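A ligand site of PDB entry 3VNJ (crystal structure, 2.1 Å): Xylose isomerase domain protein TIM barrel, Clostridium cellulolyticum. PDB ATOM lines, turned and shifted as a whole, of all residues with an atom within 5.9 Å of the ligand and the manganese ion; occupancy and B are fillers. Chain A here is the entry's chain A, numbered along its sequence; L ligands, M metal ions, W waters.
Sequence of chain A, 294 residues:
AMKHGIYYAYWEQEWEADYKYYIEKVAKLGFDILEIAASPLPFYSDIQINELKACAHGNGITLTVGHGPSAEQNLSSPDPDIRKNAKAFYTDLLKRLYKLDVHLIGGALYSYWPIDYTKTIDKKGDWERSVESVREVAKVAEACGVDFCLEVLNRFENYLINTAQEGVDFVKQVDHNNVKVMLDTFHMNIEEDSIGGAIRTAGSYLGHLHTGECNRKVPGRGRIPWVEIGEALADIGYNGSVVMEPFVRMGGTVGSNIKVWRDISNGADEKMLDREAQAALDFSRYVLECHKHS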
ATOM      1  N   TYR A   7       8.829 -16.271  15.572  1.00  0.00           N
ATOM      2  CA  TYR A   7       7.725 -15.893  16.427  1.00  0.00           C
ATOM      3  C   TYR A   7       7.644 -16.960  17.553  1.00  0.00           C
ATOM      4  O   TYR A   7       7.631 -18.157  17.257  1.00  0.00           O
ATOM      5  CB  TYR A   7       6.464 -15.850  15.580  1.00  0.00           C
ATOM      6  CG  TYR A   7       5.239 -15.232  16.193  1.00  0.00           C
ATOM      7  CD1 TYR A   7       5.345 -14.281  17.196  1.00  0.00           C
ATOM      8  CD2 TYR A   7       3.978 -15.507  15.678  1.00  0.00           C
ATOM      9  CE1 TYR A   7       4.209 -13.591  17.690  1.00  0.00           C
ATOM     10  CE2 TYR A   7       2.811 -14.822  16.142  1.00  0.00           C
ATOM     11  CZ  TYR A   7       2.955 -13.855  17.159  1.00  0.00           C
ATOM     12  OH  TYR A   7       1.860 -13.156  17.612  1.00  0.00           O
ATOM     13  N   TRP A  15      -1.876 -16.587  22.813  1.00  0.00           N
ATOM     14  CA  TRP A  15      -1.161 -15.376  22.416  1.00  0.00           C
ATOM     15  C   TRP A  15      -0.416 -14.705  23.579  1.00  0.00           C
ATOM     16  O   TRP A  15      -0.479 -13.488  23.768  1.00  0.00           O
ATOM     17  CB  TRP A  15      -2.120 -14.379  21.712  1.00  0.00           C
ATOM     18  CG  TRP A  15      -2.682 -14.934  20.423  1.00  0.00           C
ATOM     19  CD1 TRP A  15      -4.007 -15.118  20.126  1.00  0.00           C
ATOM     20  CD2 TRP A  15      -1.945 -15.397  19.262  1.00  0.00           C
ATOM     21  NE1 TRP A  15      -4.145 -15.665  18.878  1.00  0.00           N
ATOM     22  CE2 TRP A  15      -2.900 -15.852  18.320  1.00  0.00           C
ATOM     23  CE3 TRP A  15      -0.580 -15.486  18.942  1.00  0.00           C
ATOM     24  CZ2 TRP A  15      -2.545 -16.396  17.060  1.00  0.00           C
ATOM     25  CZ3 TRP A  15      -0.213 -16.025  17.689  1.00  0.00           C
ATOM     26  CH2 TRP A  15      -1.200 -16.473  16.765  1.00  0.00           C
ATOM     27  N   GLU A  35      10.206 -12.674  18.180  1.00  0.00           N
ATOM     28  CA  GLU A  35       9.026 -11.815  18.010  1.00  0.00           C
ATOM     29  C   GLU A  35       8.045 -12.322  19.042  1.00  0.00           C
ATOM     30  O   GLU A  35       7.875 -13.544  19.218  1.00  0.00           O
ATOM     31  CB  GLU A  35       8.433 -11.929  16.607  1.00  0.00           C
ATOM     32  CG  GLU A  35       7.190 -11.005  16.366  1.00  0.00           C
ATOM     33  CD  GLU A  35       7.042 -10.601  14.868  1.00  0.00           C
ATOM     34  OE1 GLU A  35       8.040 -10.095  14.311  1.00  0.00           O
ATOM     35  OE2 GLU A  35       5.938 -10.781  14.292  1.00  0.00           O
ATOM     36  N   ALA A  37       4.078 -11.787  21.090  1.00  0.00           N
ATOM     37  CA  ALA A  37       2.713 -11.266  20.928  1.00  0.00           C
ATOM     38  C   ALA A  37       2.507 -10.086  21.885  1.00  0.00           C
ATOM     39  O   ALA A  37       2.978 -10.125  23.052  1.00  0.00           O
ATOM     40  CB  ALA A  37       1.671 -12.370  21.238  1.00  0.00           C
ATOM     41  N   GLY A  66       4.302  -8.588  17.339  1.00  0.00           N
ATOM     42  CA  GLY A  66       3.252  -8.856  16.385  1.00  0.00           C
ATOM     43  C   GLY A  66       1.955  -8.676  17.163  1.00  0.00           C
ATOM     44  O   GLY A  66       1.922  -8.918  18.376  1.00  0.00           O
ATOM     45  N   HIS A  67       0.879  -8.234  16.508  1.00  0.00           N
ATOM     46  CA  HIS A  67      -0.407  -8.106  17.200  1.00  0.00           C
ATOM     47  C   HIS A  67      -1.618  -8.356  16.284  1.00  0.00           C
ATOM     48  O   HIS A  67      -1.740  -7.735  15.222  1.00  0.00           O
ATOM     49  CB  HIS A  67      -0.560  -6.705  17.858  1.00  0.00           C
ATOM     50  CG  HIS A  67      -1.772  -6.602  18.745  1.00  0.00           C
ATOM     51  ND1 HIS A  67      -2.080  -7.563  19.684  1.00  0.00           N
ATOM     52  CD2 HIS A  67      -2.745  -5.664  18.835  1.00  0.00           C
ATOM     53  CE1 HIS A  67      -3.184  -7.226  20.315  1.00  0.00           C
ATOM     54  NE2 HIS A  67      -3.616  -6.075  19.824  1.00  0.00           N
ATOM     55  N   GLY A  68      -2.469  -9.304  16.641  1.00  0.00           N
ATOM     56  CA  GLY A  68      -3.678  -9.508  15.861  1.00  0.00           C
ATOM     57  C   GLY A  68      -4.683  -8.732  16.717  1.00  0.00           C
ATOM     58  O   GLY A  68      -5.043  -9.230  17.780  1.00  0.00           O
ATOM     59  N   GLY A 106       3.914  -5.110  14.267  1.00  0.00           N
ATOM     60  CA  GLY A 106       3.346  -5.424  12.965  1.00  0.00           C
ATOM     61  C   GLY A 106       2.159  -6.335  13.066  1.00  0.00           C
ATOM     62  O   GLY A 106       1.923  -6.957  14.119  1.00  0.00           O
ATOM     63  N   GLY A 107       1.419  -6.450  11.975  1.00  0.00           N
ATOM     64  CA  GLY A 107       0.221  -7.293  11.952  1.00  0.00           C
ATOM     65  C   GLY A 107      -0.902  -6.502  11.266  1.00  0.00           C
ATOM     66  O   GLY A 107      -0.630  -5.530  10.567  1.00  0.00           O
ATOM     67  N   ALA A 108      -2.165  -6.889  11.460  1.00  0.00           N
ATOM     68  CA  ALA A 108      -3.272  -6.178  10.815  1.00  0.00           C
ATOM     69  C   ALA A 108      -3.623  -4.976  11.689  1.00  0.00           C
ATOM     70  O   ALA A 108      -4.745  -4.858  12.171  1.00  0.00           O
ATOM     71  CB  ALA A 108      -4.463  -7.090  10.681  1.00  0.00           C
ATOM     72  N   TRP A 113      -8.182  -8.834  13.834  1.00  0.00           N
ATOM     73  CA  TRP A 113      -7.887 -10.153  13.281  1.00  0.00           C
ATOM     74  C   TRP A 113      -8.048 -11.180  14.389  1.00  0.00           C
ATOM     75  O   TRP A 113      -7.550 -10.990  15.497  1.00  0.00           O
ATOM     76  CB  TRP A 113      -6.418 -10.184  12.837  1.00  0.00           C
ATOM     77  CG  TRP A 113      -5.889 -11.536  12.398  1.00  0.00           C
ATOM     78  CD1 TRP A 113      -5.876 -12.042  11.125  1.00  0.00           C
ATOM     79  CD2 TRP A 113      -5.330 -12.563  13.238  1.00  0.00           C
ATOM     80  NE1 TRP A 113      -5.352 -13.305  11.108  1.00  0.00           N
ATOM     81  CE2 TRP A 113      -4.994 -13.662  12.392  1.00  0.00           C
ATOM     82  CE3 TRP A 113      -5.076 -12.670  14.615  1.00  0.00           C
ATOM     83  CZ2 TRP A 113      -4.419 -14.858  12.885  1.00  0.00           C
ATOM     84  CZ3 TRP A 113      -4.495 -13.876  15.117  1.00  0.00           C
ATOM     85  CH2 TRP A 113      -4.177 -14.947  14.244  1.00  0.00           C
ATOM     86  N   GLU A 151       0.616  -5.328   7.785  1.00  0.00           N
ATOM     87  CA  GLU A 151       0.756  -6.609   7.117  1.00  0.00           C
ATOM     88  C   GLU A 151      -0.311  -6.930   6.119  1.00  0.00           C
ATOM     89  O   GLU A 151      -1.490  -6.923   6.421  1.00  0.00           O
ATOM     90  CB  GLU A 151       0.817  -7.757   8.142  1.00  0.00           C
ATOM     91  CG  GLU A 151       0.937  -9.146   7.531  1.00  0.00           C
ATOM     92  CD  GLU A 151       1.174 -10.245   8.625  1.00  0.00           C
ATOM     93  OE1 GLU A 151       0.986  -9.998   9.823  1.00  0.00           O
ATOM     94  OE2 GLU A 151       1.538 -11.363   8.270  1.00  0.00           O
ATOM     95  N   LEU A 153      -2.481  -9.340   4.215  1.00  0.00           N
ATOM     96  CA  LEU A 153      -2.984 -10.667   4.527  1.00  0.00           C
ATOM     97  C   LEU A 153      -3.838 -11.236   3.443  1.00  0.00           C
ATOM     98  O   LEU A 153      -4.339 -10.468   2.586  1.00  0.00           O
ATOM     99  CB  LEU A 153      -3.832 -10.601   5.787  1.00  0.00           C
ATOM    100  CG  LEU A 153      -3.176 -10.056   7.069  1.00  0.00           C
ATOM    101  CD1 LEU A 153      -4.238 -10.013   8.132  1.00  0.00           C
ATOM    102  CD2 LEU A 153      -2.047 -10.953   7.527  1.00  0.00           C
ATOM    103  N   ASN A 154      -4.064 -12.559   3.472  1.00  0.00           N
ATOM    104  CA  ASN A 154      -4.893 -13.154   2.458  1.00  0.00           C
ATOM    105  C   ASN A 154      -6.370 -12.841   2.761  1.00  0.00           C
ATOM    106  O   ASN A 154      -6.759 -12.470   3.885  1.00  0.00           O
ATOM    107  CB  ASN A 154      -4.647 -14.664   2.358  1.00  0.00           C
ATOM    108  CG  ASN A 154      -5.132 -15.415   3.578  1.00  0.00           C
ATOM    109  OD1 ASN A 154      -6.340 -15.528   3.809  1.00  0.00           O
ATOM    110  ND2 ASN A 154      -4.176 -15.942   4.395  1.00  0.00           N
ATOM    111  N   GLU A 157      -8.508 -13.827   5.896  1.00  0.00           N
ATOM    112  CA  GLU A 157      -8.191 -13.250   7.201  1.00  0.00           C
ATOM    113  C   GLU A 157      -8.489 -11.777   7.331  1.00  0.00           C
ATOM    114  O   GLU A 157      -8.632 -11.265   8.438  1.00  0.00           O
ATOM    115  CB  GLU A 157      -6.722 -13.548   7.540  1.00  0.00           C
ATOM    116  CG  GLU A 157      -6.490 -15.035   7.722  1.00  0.00           C
ATOM    117  CD  GLU A 157      -5.073 -15.376   8.164  1.00  0.00           C
ATOM    118  OE1 GLU A 157      -4.514 -14.722   9.095  1.00  0.00           O
ATOM    119  OE2 GLU A 157      -4.514 -16.312   7.552  1.00  0.00           O
ATOM    120  N   MET A 182       4.237  -4.589   5.226  1.00  0.00           N
ATOM    121  CA  MET A 182       4.851  -5.814   5.754  1.00  0.00           C
ATOM    122  C   MET A 182       4.264  -6.924   4.928  1.00  0.00           C
ATOM    123  O   MET A 182       3.067  -6.973   4.743  1.00  0.00           O
ATOM    124  CB  MET A 182       4.503  -5.976   7.229  1.00  0.00           C
ATOM    125  CG  MET A 182       4.654  -7.360   7.878  1.00  0.00           C
ATOM    126  SD  MET A 182       4.235  -7.156   9.661  1.00  0.00           S
ATOM    127  CE  MET A 182       4.263  -9.002  10.203  1.00  0.00           C
ATOM    128  N   ASP A 184       4.295 -11.309   3.969  1.00  0.00           N
ATOM    129  CA  ASP A 184       4.398 -12.592   4.644  1.00  0.00           C
ATOM    130  C   ASP A 184       4.263 -13.643   3.531  1.00  0.00           C
ATOM    131  O   ASP A 184       3.259 -13.691   2.857  1.00  0.00           O
ATOM    132  CB  ASP A 184       3.223 -12.688   5.626  1.00  0.00           C
ATOM    133  CG  ASP A 184       3.051 -14.064   6.274  1.00  0.00           C
ATOM    134  OD1 ASP A 184       3.274 -15.140   5.618  1.00  0.00           O
ATOM    135  OD2 ASP A 184       2.603 -14.056   7.454  1.00  0.00           O
ATOM    136  N   PHE A 186       3.427 -16.650   3.459  1.00  0.00           N
ATOM    137  CA  PHE A 186       2.224 -17.514   3.496  1.00  0.00           C
ATOM    138  C   PHE A 186       0.993 -16.789   2.848  1.00  0.00           C
ATOM    139  O   PHE A 186       0.163 -17.414   2.173  1.00  0.00           O
ATOM    140  CB  PHE A 186       1.875 -17.897   4.944  1.00  0.00           C
ATOM    141  CG  PHE A 186       0.488 -18.457   5.119  1.00  0.00           C
ATOM    142  CD1 PHE A 186       0.185 -19.761   4.690  1.00  0.00           C
ATOM    143  CD2 PHE A 186      -0.512 -17.698   5.705  1.00  0.00           C
ATOM    144  CE1 PHE A 186      -1.071 -20.271   4.852  1.00  0.00           C
ATOM    145  CE2 PHE A 186      -1.773 -18.190   5.878  1.00  0.00           C
ATOM    146  CZ  PHE A 186      -2.050 -19.514   5.432  1.00  0.00           C
ATOM    147  N   HIS A 187       0.910 -15.484   3.051  1.00  0.00           N
ATOM    148  CA  HIS A 187      -0.199 -14.688   2.530  1.00  0.00           C
ATOM    149  C   HIS A 187       0.034 -14.307   1.046  1.00  0.00           C
ATOM    150  O   HIS A 187      -0.903 -14.303   0.268  1.00  0.00           O
ATOM    151  CB  HIS A 187      -0.399 -13.446   3.379  1.00  0.00           C
ATOM    152  CG  HIS A 187      -0.849 -13.744   4.780  1.00  0.00           C
ATOM    153  ND1 HIS A 187      -2.064 -14.306   5.052  1.00  0.00           N
ATOM    154  CD2 HIS A 187      -0.222 -13.584   5.972  1.00  0.00           C
ATOM    155  CE1 HIS A 187      -2.196 -14.472   6.355  1.00  0.00           C
ATOM    156  NE2 HIS A 187      -1.087 -14.038   6.946  1.00  0.00           N
ATOM    157  N   HIS A 210       7.576 -11.653   7.209  1.00  0.00           N
ATOM    158  CA  HIS A 210       7.269 -12.887   7.928  1.00  0.00           C
ATOM    159  C   HIS A 210       7.489 -14.067   6.950  1.00  0.00           C
ATOM    160  O   HIS A 210       7.108 -13.999   5.764  1.00  0.00           O
ATOM    161  CB  HIS A 210       5.807 -12.924   8.340  1.00  0.00           C
ATOM    162  CG  HIS A 210       5.484 -12.331   9.687  1.00  0.00           C
ATOM    163  ND1 HIS A 210       4.186 -12.225  10.139  1.00  0.00           N
ATOM    164  CD2 HIS A 210       6.258 -11.803  10.658  1.00  0.00           C
ATOM    165  CE1 HIS A 210       4.186 -11.657  11.332  1.00  0.00           C
ATOM    166  NE2 HIS A 210       5.424 -11.384  11.668  1.00  0.00           N
ATOM    167  N   ARG A 216       2.413 -23.304   6.231  1.00  0.00           N
ATOM    168  CA  ARG A 216       3.015 -22.772   7.468  1.00  0.00           C
ATOM    169  C   ARG A 216       4.064 -23.573   8.194  1.00  0.00           C
ATOM    170  O   ARG A 216       4.278 -23.360   9.380  1.00  0.00           O
ATOM    171  CB  ARG A 216       1.943 -22.397   8.491  1.00  0.00           C
ATOM    172  CG  ARG A 216       0.858 -21.430   7.997  1.00  0.00           C
ATOM    173  CD  ARG A 216       1.212 -19.979   8.423  1.00  0.00           C
ATOM    174  NE  ARG A 216      -0.022 -19.326   8.694  1.00  0.00           N
ATOM    175  CZ  ARG A 216      -0.174 -18.039   8.960  1.00  0.00           C
ATOM    176  NH1 ARG A 216       0.853 -17.207   8.995  1.00  0.00           N
ATOM    177  NH2 ARG A 216      -1.398 -17.611   9.191  1.00  0.00           N
ATOM    178  N   GLU A 245       7.493 -17.560  10.952  1.00  0.00           N
ATOM    179  CA  GLU A 245       6.306 -17.654  11.775  1.00  0.00           C
ATOM    180  C   GLU A 245       5.676 -19.058  11.539  1.00  0.00           C
ATOM    181  O   GLU A 245       4.562 -19.162  11.037  1.00  0.00           O
ATOM    182  CB  GLU A 245       5.361 -16.527  11.311  1.00  0.00           C
ATOM    183  CG  GLU A 245       4.218 -16.194  12.234  1.00  0.00           C
ATOM    184  CD  GLU A 245       3.347 -15.051  11.658  1.00  0.00           C
ATOM    185  OE1 GLU A 245       3.131 -15.041  10.447  1.00  0.00           O
ATOM    186  OE2 GLU A 245       2.894 -14.182  12.421  1.00  0.00           O
ATOM    187  N   PHE A 247       3.592 -22.448  12.162  1.00  0.00           N
ATOM    188  CA  PHE A 247       2.470 -22.821  13.022  1.00  0.00           C
ATOM    189  C   PHE A 247       2.220 -24.273  12.638  1.00  0.00           C
ATOM    190  O   PHE A 247       1.596 -24.564  11.601  1.00  0.00           O
ATOM    191  CB  PHE A 247       1.197 -22.002  12.759  1.00  0.00           C
ATOM    192  CG  PHE A 247       1.279 -20.529  13.164  1.00  0.00           C
ATOM    193  CD1 PHE A 247       1.211 -20.163  14.496  1.00  0.00           C
ATOM    194  CD2 PHE A 247       1.426 -19.541  12.203  1.00  0.00           C
ATOM    195  CE1 PHE A 247       1.310 -18.806  14.904  1.00  0.00           C
ATOM    196  CE2 PHE A 247       1.534 -18.199  12.579  1.00  0.00           C
ATOM    197  CZ  PHE A 247       1.473 -17.831  13.954  1.00  0.00           C
ATOM    198  N   ILE A 258      -5.304 -19.719  13.679  1.00  0.00           N
ATOM    199  CA  ILE A 258      -4.478 -20.020  12.516  1.00  0.00           C
ATOM    200  C   ILE A 258      -5.079 -21.141  11.677  1.00  0.00           C
ATOM    201  O   ILE A 258      -4.670 -21.361  10.539  1.00  0.00           O
ATOM    202  CB  ILE A 258      -3.032 -20.363  12.981  1.00  0.00           C
ATOM    203  CG1 ILE A 258      -2.475 -19.142  13.718  1.00  0.00           C
ATOM    204  CG2 ILE A 258      -2.135 -20.758  11.807  1.00  0.00           C
ATOM    205  CD1 ILE A 258      -2.175 -17.926  12.814  1.00  0.00           C
HETATM  206  C1  LIG L   1      -1.685 -14.172  10.797  1.00  0.00           C
HETATM  207  O1  LIG L   1      -2.110 -14.995   9.712  1.00  0.00           O
HETATM  208  C2  LIG L   1      -0.354 -13.482  10.457  1.00  0.00           C
HETATM  209  O2  LIG L   1       0.392 -13.864   9.579  1.00  0.00           O
HETATM  210  C3  LIG L   1      -0.056 -12.191  11.239  1.00  0.00           C
HETATM  211  O3  LIG L   1       1.350 -12.149  11.467  1.00  0.00           O
HETATM  212  C4  LIG L   1      -0.804 -12.151  12.573  1.00  0.00           C
HETATM  213  O4  LIG L   1      -0.884 -10.810  13.050  1.00  0.00           O
HETATM  214  C5  LIG L   1      -0.050 -12.958  13.637  1.00  0.00           C
HETATM  215  O5  LIG L   1       0.145 -14.298  13.196  1.00  0.00           O
HETATM  216  C6  LIG L   1      -0.899 -12.890  14.911  1.00  0.00           C
HETATM  217  O6  LIG L   1      -0.170 -13.368  16.042  1.00  0.00           O
HETATM  218 MN    MN M   1       2.354 -13.079   9.389  1.00  0.00          MN
HETATM  219  O   HOH W   1       1.690  -9.874  13.443  1.00  0.00           O
HETATM  220  O   HOH W   2      -1.840 -11.863  18.290  1.00  0.00           O
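NH2 of Arg 216 sits at hydrogen-bond distance from O1 of the ligand (2.8 Å). NE2 of His 187 sits at hydrogen-bond distance from O1 of the ligand (3.1 Å). An oxygen (O6) of the ligand lies within hydrogen-bond range of the side-chain hydroxyl (OH) of Tyr 7, 2.6 Å away. An oxygen (O1) of the ligand lies within hydrogen-bond range of the side-chain carboxylate (OE1) of Glu 157, 2.5 Å away.
Within 4 Å of the manganese ion: Glu 151, Asp 184, His 210 and Glu 245.
Water W1 lies within hydrogen-bond range of an oxygen (O4) of the ligand (2.8 Å) and the backbone carbonyl oxygen of Gly 106 (3.0 Å). Water W2 lies within hydrogen-bond range of the backbone NH of Gly 68 (3.1 Å) and an oxygen (O6) of the ligand (3.2 Å).
Residues that only touch the ligand: Trp 15 (3.1 Å), His 67 (3.9 Å), Gly 107 (3.8 Å), Trp 113 (3.5 Å) and Phe 247 (3.8 Å). Hydrophobic or aromatic side chains that line the ligand: Tyr 7, Trp 15, Trp 113, His 187, His 210 and Phe 247. 13 residues have an atom within 4 Å of the ligand: Tyr 7, Trp 15, His 67, Gly 107, Trp 113, Glu 151, Glu 157, Asp 184, His 187, His 210, Arg 216, Glu 245 and Phe 247. The nearest printed residue that does not touch the ligand is Gly 68 (4.2 Å).
O2 of the ligand binds the manganese ion, 2.1 Å away. ND1 of His 210 binds the manganese ion (2.2 Å). The manganese ion is bound by the side-chain carboxylate (OD2) of Asp 184 (2.2 Å). OE2 of Glu 151 is bound to the manganese ion (2.2 Å). The side-chain carboxylate (OE1) of Glu 245 is bound to the manganese ion. The manganese ion is bound by an oxygen (O3) of the ligand (2.5 Å). The manganese ion has six donor atoms within binding distance.
The backbone carbonyl oxygen (O) of Arg 216 sits at hydrogen-bond distance from the backbone NH (N) of Phe 247 (3.0 Å). The side-chain carboxylate of Glu 157 sits at hydrogen-bond distance from the side-chain amide nitrogen of Asn 154 (3.2 Å). ND1 of His 187 is in hydrogen-bond range of ND2 of Asn 154, 2.8 Å away. The side-chain sulfur (SD) of Met 182 is in hydrogen-bond range of the backbone NH (N) of Gly 107, at 3.7 Å. The backbone carbonyl oxygen (O) of Gly 107 is in hydrogen-bond range of the backbone NH (N) of Glu 151 (3.1 Å). The backbone NH (N) of His 67 sits at hydrogen-bond distance from the backbone carbonyl oxygen (O) of Gly 106. OE2 of Glu 35 sits at hydrogen-bond distance from NE2 of His 210. The side-chain carboxylate (OE1) of Glu 245 lies close to the guanidinium group (NH1) of Arg 216, at 3.5 Å.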
